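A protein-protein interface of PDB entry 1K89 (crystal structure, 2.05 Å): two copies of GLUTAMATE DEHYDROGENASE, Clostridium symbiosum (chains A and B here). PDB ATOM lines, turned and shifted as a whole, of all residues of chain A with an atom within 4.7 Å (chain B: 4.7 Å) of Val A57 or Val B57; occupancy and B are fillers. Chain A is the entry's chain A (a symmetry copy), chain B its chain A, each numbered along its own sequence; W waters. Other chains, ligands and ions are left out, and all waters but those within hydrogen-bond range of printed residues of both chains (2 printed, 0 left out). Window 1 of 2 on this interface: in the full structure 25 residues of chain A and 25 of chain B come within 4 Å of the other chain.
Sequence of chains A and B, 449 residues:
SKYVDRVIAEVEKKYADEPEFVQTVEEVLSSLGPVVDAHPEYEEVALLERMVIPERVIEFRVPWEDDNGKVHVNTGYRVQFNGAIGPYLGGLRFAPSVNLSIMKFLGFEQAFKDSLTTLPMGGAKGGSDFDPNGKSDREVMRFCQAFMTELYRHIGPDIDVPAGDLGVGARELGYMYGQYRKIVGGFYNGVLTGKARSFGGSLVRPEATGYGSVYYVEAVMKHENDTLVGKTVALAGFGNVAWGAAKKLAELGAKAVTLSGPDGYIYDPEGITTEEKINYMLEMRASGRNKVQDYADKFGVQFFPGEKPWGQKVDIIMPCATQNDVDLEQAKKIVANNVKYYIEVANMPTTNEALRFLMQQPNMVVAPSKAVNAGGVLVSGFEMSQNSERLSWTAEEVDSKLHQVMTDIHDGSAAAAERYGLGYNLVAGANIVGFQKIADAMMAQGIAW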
ATOM      1  N   PRO A  54     -21.503  19.028  -0.487  1.00  0.00           N
ATOM      2  CA  PRO A  54     -22.588  18.613   0.397  1.00  0.00           C
ATOM      3  C   PRO A  54     -22.059  18.448   1.830  1.00  0.00           C
ATOM      4  O   PRO A  54     -20.910  18.030   2.055  1.00  0.00           O
ATOM      5  CB  PRO A  54     -23.052  17.248  -0.163  1.00  0.00           C
ATOM      6  CG  PRO A  54     -22.302  16.989  -1.382  1.00  0.00           C
ATOM      7  CD  PRO A  54     -21.147  17.997  -1.475  1.00  0.00           C
ATOM      8  N   GLU A  55     -22.899  18.770   2.808  1.00  0.00           N
ATOM      9  CA  GLU A  55     -22.490  18.562   4.217  1.00  0.00           C
ATOM     10  C   GLU A  55     -22.115  17.127   4.430  1.00  0.00           C
ATOM     11  O   GLU A  55     -21.099  16.807   5.046  1.00  0.00           O
ATOM     12  CB  GLU A  55     -23.659  18.952   5.158  1.00  0.00           C
ATOM     13  CG  GLU A  55     -23.803  20.525   5.187  1.00  0.00           C
ATOM     14  CD  GLU A  55     -24.944  21.015   6.009  1.00  0.00           C
ATOM     15  OE1 GLU A  55     -25.424  20.258   6.876  1.00  0.00           O
ATOM     16  OE2 GLU A  55     -25.286  22.209   5.912  1.00  0.00           O
ATOM     17  N   ARG A  56     -22.963  16.225   3.935  1.00  0.00           N
ATOM     18  CA  ARG A  56     -22.749  14.805   4.175  1.00  0.00           C
ATOM     19  C   ARG A  56     -23.303  14.004   2.981  1.00  0.00           C
ATOM     20  O   ARG A  56     -24.372  14.331   2.459  1.00  0.00           O
ATOM     21  CB  ARG A  56     -23.549  14.477   5.446  1.00  0.00           C
ATOM     22  CG  ARG A  56     -23.213  13.184   6.023  1.00  0.00           C
ATOM     23  CD  ARG A  56     -24.147  12.881   7.196  1.00  0.00           C
ATOM     24  NE  ARG A  56     -23.799  13.713   8.345  1.00  0.00           N
ATOM     25  CZ  ARG A  56     -24.535  14.715   8.803  1.00  0.00           C
ATOM     26  NH1 ARG A  56     -25.698  15.053   8.229  1.00  0.00           N
ATOM     27  NH2 ARG A  56     -24.093  15.403   9.850  1.00  0.00           N
ATOM     28  N   VAL A  57     -22.538  13.005   2.528  1.00  0.00           N
ATOM     29  CA  VAL A  57     -22.966  12.078   1.459  1.00  0.00           C
ATOM     30  C   VAL A  57     -22.984  10.637   2.052  1.00  0.00           C
ATOM     31  O   VAL A  57     -22.016  10.208   2.668  1.00  0.00           O
ATOM     32  CB  VAL A  57     -21.998  12.084   0.224  1.00  0.00           C
ATOM     33  CG1 VAL A  57     -22.278  10.926  -0.678  1.00  0.00           C
ATOM     34  CG2 VAL A  57     -22.172  13.318  -0.576  1.00  0.00           C
ATOM     35  N   ILE A  58     -24.053   9.871   1.869  1.00  0.00           N
ATOM     36  CA  ILE A  58     -24.040   8.474   2.356  1.00  0.00           C
ATOM     37  C   ILE A  58     -24.377   7.583   1.161  1.00  0.00           C
ATOM     38  O   ILE A  58     -25.342   7.873   0.458  1.00  0.00           O
ATOM     39  CB  ILE A  58     -25.121   8.193   3.495  1.00  0.00           C
ATOM     40  CG1 ILE A  58     -24.889   9.046   4.742  1.00  0.00           C
ATOM     41  CG2 ILE A  58     -25.102   6.694   3.973  1.00  0.00           C
ATOM     42  CD1 ILE A  58     -26.133   9.864   5.088  1.00  0.00           C
ATOM     43  N   GLU A  59     -23.584   6.532   0.930  1.00  0.00           N
ATOM     44  CA  GLU A  59     -23.887   5.559  -0.118  1.00  0.00           C
ATOM     45  C   GLU A  59     -23.845   4.252   0.635  1.00  0.00           C
ATOM     46  O   GLU A  59     -22.972   4.070   1.509  1.00  0.00           O
ATOM     47  CB  GLU A  59     -22.779   5.454  -1.177  1.00  0.00           C
ATOM     48  CG  GLU A  59     -22.467   6.724  -1.895  1.00  0.00           C
ATOM     49  CD  GLU A  59     -21.627   6.515  -3.155  1.00  0.00           C
ATOM     50  OE1 GLU A  59     -21.398   5.274  -3.532  1.00  0.00           O
ATOM     51  OE2 GLU A  59     -21.335   7.466  -3.844  1.00  0.00           O
ATOM     52  N   ARG A  78     -27.858   8.894  -0.236  1.00  0.00           N
ATOM     53  CA  ARG A  78     -28.562  10.037   0.383  1.00  0.00           C
ATOM     54  C   ARG A  78     -27.480  11.138   0.447  1.00  0.00           C
ATOM     55  O   ARG A  78     -26.477  11.008   1.168  1.00  0.00           O
ATOM     56  CB  ARG A  78     -29.169   9.783   1.795  1.00  0.00           C
ATOM     57  CG  ARG A  78     -30.018  11.039   2.311  1.00  0.00           C
ATOM     58  CD  ARG A  78     -31.324  11.149   1.537  1.00  0.00           C
ATOM     59  NE  ARG A  78     -32.245  12.143   2.066  1.00  0.00           N
ATOM     60  CZ  ARG A  78     -33.294  12.601   1.387  1.00  0.00           C
ATOM     61  NH1 ARG A  78     -33.525  12.164   0.130  1.00  0.00           N
ATOM     62  NH2 ARG A  78     -34.102  13.509   1.935  1.00  0.00           N
ATOM     63  N   VAL A  79     -27.736  12.234  -0.237  1.00  0.00           N
ATOM     64  CA  VAL A  79     -26.835  13.339  -0.247  1.00  0.00           C
ATOM     65  C   VAL A  79     -27.528  14.394   0.611  1.00  0.00           C
ATOM     66  O   VAL A  79     -28.563  14.931   0.226  1.00  0.00           O
ATOM     67  CB  VAL A  79     -26.710  13.862  -1.692  1.00  0.00           C
ATOM     68  CG1 VAL A  79     -25.897  15.152  -1.709  1.00  0.00           C
ATOM     69  CG2 VAL A  79     -25.973  12.818  -2.580  1.00  0.00           C
ATOM     70  N   LEU A 100     -24.041   9.138  -8.162  1.00  0.00           N
ATOM     71  CA  LEU A 100     -23.741  10.268  -7.294  1.00  0.00           C
ATOM     72  C   LEU A 100     -23.911  11.597  -8.044  1.00  0.00           C
ATOM     73  O   LEU A 100     -24.572  12.528  -7.543  1.00  0.00           O
ATOM     74  CB  LEU A 100     -22.338  10.115  -6.694  1.00  0.00           C
ATOM     75  CG  LEU A 100     -22.016  11.242  -5.699  1.00  0.00           C
ATOM     76  CD1 LEU A 100     -23.035  11.184  -4.507  1.00  0.00           C
ATOM     77  CD2 LEU A 100     -20.562  11.137  -5.205  1.00  0.00           C
ATOM     78  N   PRO B  54     -19.033  -1.445  -1.035  1.00  0.00           N
ATOM     79  CA  PRO B  54     -18.810  -1.195   0.386  1.00  0.00           C
ATOM     80  C   PRO B  54     -20.153  -1.188   1.132  1.00  0.00           C
ATOM     81  O   PRO B  54     -21.189  -0.748   0.601  1.00  0.00           O
ATOM     82  CB  PRO B  54     -18.157   0.206   0.441  1.00  0.00           C
ATOM     83  CG  PRO B  54     -17.941   0.650  -0.927  1.00  0.00           C
ATOM     84  CD  PRO B  54     -18.706  -0.283  -1.877  1.00  0.00           C
ATOM     85  N   GLU B  55     -20.141  -1.668   2.369  1.00  0.00           N
ATOM     86  CA  GLU B  55     -21.380  -1.620   3.181  1.00  0.00           C
ATOM     87  C   GLU B  55     -21.870  -0.207   3.276  1.00  0.00           C
ATOM     88  O   GLU B  55     -23.055   0.081   3.113  1.00  0.00           O
ATOM     89  CB  GLU B  55     -21.092  -2.180   4.599  1.00  0.00           C
ATOM     90  CG  GLU B  55     -20.929  -3.749   4.517  1.00  0.00           C
ATOM     91  CD  GLU B  55     -20.580  -4.391   5.814  1.00  0.00           C
ATOM     92  OE1 GLU B  55     -20.817  -3.773   6.870  1.00  0.00           O
ATOM     93  OE2 GLU B  55     -20.201  -5.578   5.815  1.00  0.00           O
ATOM     94  N   ARG B  56     -20.948   0.710   3.573  1.00  0.00           N
ATOM     95  CA  ARG B  56     -21.333   2.096   3.791  1.00  0.00           C
ATOM     96  C   ARG B  56     -20.172   3.014   3.361  1.00  0.00           C
ATOM     97  O   ARG B  56     -19.008   2.705   3.628  1.00  0.00           O
ATOM     98  CB  ARG B  56     -21.573   2.224   5.304  1.00  0.00           C
ATOM     99  CG  ARG B  56     -22.265   3.449   5.678  1.00  0.00           C
ATOM    100  CD  ARG B  56     -22.339   3.557   7.201  1.00  0.00           C
ATOM    101  NE  ARG B  56     -23.312   2.605   7.728  1.00  0.00           N
ATOM    102  CZ  ARG B  56     -23.008   1.520   8.425  1.00  0.00           C
ATOM    103  NH1 ARG B  56     -21.738   1.203   8.713  1.00  0.00           N
ATOM    104  NH2 ARG B  56     -23.994   0.728   8.832  1.00  0.00           N
ATOM    105  N   VAL B  57     -20.502   4.096   2.649  1.00  0.00           N
ATOM    106  CA  VAL B  57     -19.523   5.129   2.246  1.00  0.00           C
ATOM    107  C   VAL B  57     -19.965   6.482   2.881  1.00  0.00           C
ATOM    108  O   VAL B  57     -21.119   6.875   2.764  1.00  0.00           O
ATOM    109  CB  VAL B  57     -19.449   5.324   0.691  1.00  0.00           C
ATOM    110  CG1 VAL B  57     -18.703   6.571   0.344  1.00  0.00           C
ATOM    111  CG2 VAL B  57     -18.738   4.194   0.052  1.00  0.00           C
ATOM    112  N   ILE B  58     -19.073   7.213   3.538  1.00  0.00           N
ATOM    113  CA  ILE B  58     -19.466   8.538   4.070  1.00  0.00           C
ATOM    114  C   ILE B  58     -18.473   9.555   3.509  1.00  0.00           C
ATOM    115  O   ILE B  58     -17.271   9.310   3.577  1.00  0.00           O
ATOM    116  CB  ILE B  58     -19.405   8.623   5.661  1.00  0.00           C
ATOM    117  CG1 ILE B  58     -20.355   7.632   6.334  1.00  0.00           C
ATOM    118  CG2 ILE B  58     -19.802  10.050   6.195  1.00  0.00           C
ATOM    119  CD1 ILE B  58     -19.603   6.719   7.302  1.00  0.00           C
ATOM    120  N   GLU B  59     -18.972  10.663   2.950  1.00  0.00           N
ATOM    121  CA  GLU B  59     -18.103  11.745   2.488  1.00  0.00           C
ATOM    122  C   GLU B  59     -18.689  12.947   3.187  1.00  0.00           C
ATOM    123  O   GLU B  59     -19.928  13.059   3.293  1.00  0.00           O
ATOM    124  CB  GLU B  59     -18.255  12.034   0.986  1.00  0.00           C
ATOM    125  CG  GLU B  59     -17.963  10.880   0.088  1.00  0.00           C
ATOM    126  CD  GLU B  59     -17.785  11.285  -1.377  1.00  0.00           C
ATOM    127  OE1 GLU B  59     -17.771  12.573  -1.652  1.00  0.00           O
ATOM    128  OE2 GLU B  59     -17.512  10.443  -2.201  1.00  0.00           O
ATOM    129  N   ARG B  78     -14.868   8.268   4.573  1.00  0.00           N
ATOM    130  CA  ARG B  78     -14.687   7.024   5.351  1.00  0.00           C
ATOM    131  C   ARG B  78     -15.495   5.977   4.555  1.00  0.00           C
ATOM    132  O   ARG B  78     -16.729   6.062   4.454  1.00  0.00           O
ATOM    133  CB  ARG B  78     -15.160   7.071   6.834  1.00  0.00           C
ATOM    134  CG  ARG B  78     -14.797   5.721   7.616  1.00  0.00           C
ATOM    135  CD  ARG B  78     -13.299   5.648   7.877  1.00  0.00           C
ATOM    136  NE  ARG B  78     -12.901   4.553   8.749  1.00  0.00           N
ATOM    137  CZ  ARG B  78     -11.643   4.136   8.869  1.00  0.00           C
ATOM    138  NH1 ARG B  78     -10.669   4.716   8.135  1.00  0.00           N
ATOM    139  NH2 ARG B  78     -11.347   3.129   9.691  1.00  0.00           N
ATOM    140  N   VAL B  79     -14.803   4.965   4.073  1.00  0.00           N
ATOM    141  CA  VAL B  79     -15.426   3.912   3.339  1.00  0.00           C
ATOM    142  C   VAL B  79     -15.412   2.727   4.299  1.00  0.00           C
ATOM    143  O   VAL B  79     -14.353   2.194   4.620  1.00  0.00           O
ATOM    144  CB  VAL B  79     -14.552   3.581   2.112  1.00  0.00           C
ATOM    145  CG1 VAL B  79     -15.095   2.343   1.407  1.00  0.00           C
ATOM    146  CG2 VAL B  79     -14.579   4.762   1.099  1.00  0.00           C
ATOM    147  N   LEU B 100     -12.568   9.201  -3.871  1.00  0.00           N
ATOM    148  CA  LEU B 100     -13.309   7.986  -3.560  1.00  0.00           C
ATOM    149  C   LEU B 100     -12.629   6.755  -4.176  1.00  0.00           C
ATOM    150  O   LEU B 100     -12.412   5.739  -3.487  1.00  0.00           O
ATOM    151  CB  LEU B 100     -14.768   8.128  -4.009  1.00  0.00           C
ATOM    152  CG  LEU B 100     -15.608   6.901  -3.617  1.00  0.00           C
ATOM    153  CD1 LEU B 100     -15.619   6.761  -2.054  1.00  0.00           C
ATOM    154  CD2 LEU B 100     -17.036   7.011  -4.184  1.00  0.00           C
HETATM  155  O   HOH W   1     -21.988   1.642  -0.706  1.00  0.00           O
HETATM  156  O   HOH W   2     -19.340  15.789   1.301  1.00  0.00           O
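Arg A56 touches Glu B59, and with the chains exchanged Glu A59 touches Arg B56. Val A57 touches its own counterpart, Val B57. Val A57 touches Ile B58, and with the chains exchanged Ile A58 touches Val B57. Val A57 touches Glu B59, and with the chains exchanged Glu A59 touches Val B57.
Water W2 lies within hydrogen-bond range of O of Pro A54 (2.8 Å) and O of Glu B59 (3.4 Å). Water W1 bridges the backbone carbonyl oxygen of Pro B54 (2.8 Å) and the backbone carbonyl oxygen of Glu A59 (3.4 Å).
N of Ile B58 sits at hydrogen-bond distance from O of Arg B78 (2.8 Å). N of Ile A58 sits at hydrogen-bond distance from O of Arg A78 (2.8 Å).
N of Val B57 sits at hydrogen-bond distance from O of Glu A59. N of Val A57 sits at hydrogen-bond distance from O of Glu B59, 2.7 Å away. The backbone carbonyl oxygen (O) of Val A57 lies close to the backbone carbonyl oxygen (O) of Val B57 (3.5 Å).
Glu A55 touches none of the printed residues of chain B. Of the printed residues of chain B, Arg A56 touches Glu B59. Val A57 touches just these residues of chain B: Val B57, Ile B58 and Glu B59. Of the printed residues of chain B, Ile A58 touches Val B57 (3.4 Å). Val A79 touches none of the printed residues of chain B. Of chain A, only Val A57 (3.5 Å), Ile A58 (3.4 Å) and Glu A59 (2.7 Å) come within 4 Å of Val B57. Of the printed residues of chain A, Ile B58 touches Val A57. Of the printed residues of chain A, Glu B59 touches Arg A56 and Val A57. The nearest printed residue of chain B that does not touch Val A57 is Arg B78 (7.0 Å). The nearest printed residue of chain A that does not touch Val B57 is Arg A78 (7.0 Å). The nearest printed residue of chain B that does not touch Glu A59 is Glu B55 (4.3 Å).
Among the printed residues, pairs that only touch across the chains: Arg A56 with Glu B59, Val A57 with Ile B58, Ile A58 with Val B57 and Glu A59 with Arg B56.
Printed residues of chain B that touch a printed residue of chain A: Arg B56, Val B57, Ile B58 and Glu B59. Of the 9 printed residues of chain A, 4 touch a printed residue of chain B. Printed residues of chain A that touch a printed residue of chain B: Arg A56, Val A57, Ile A58 and Glu A59. Along chain A the printed residues that touch a printed residue of chain B span positions 56 to 59.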
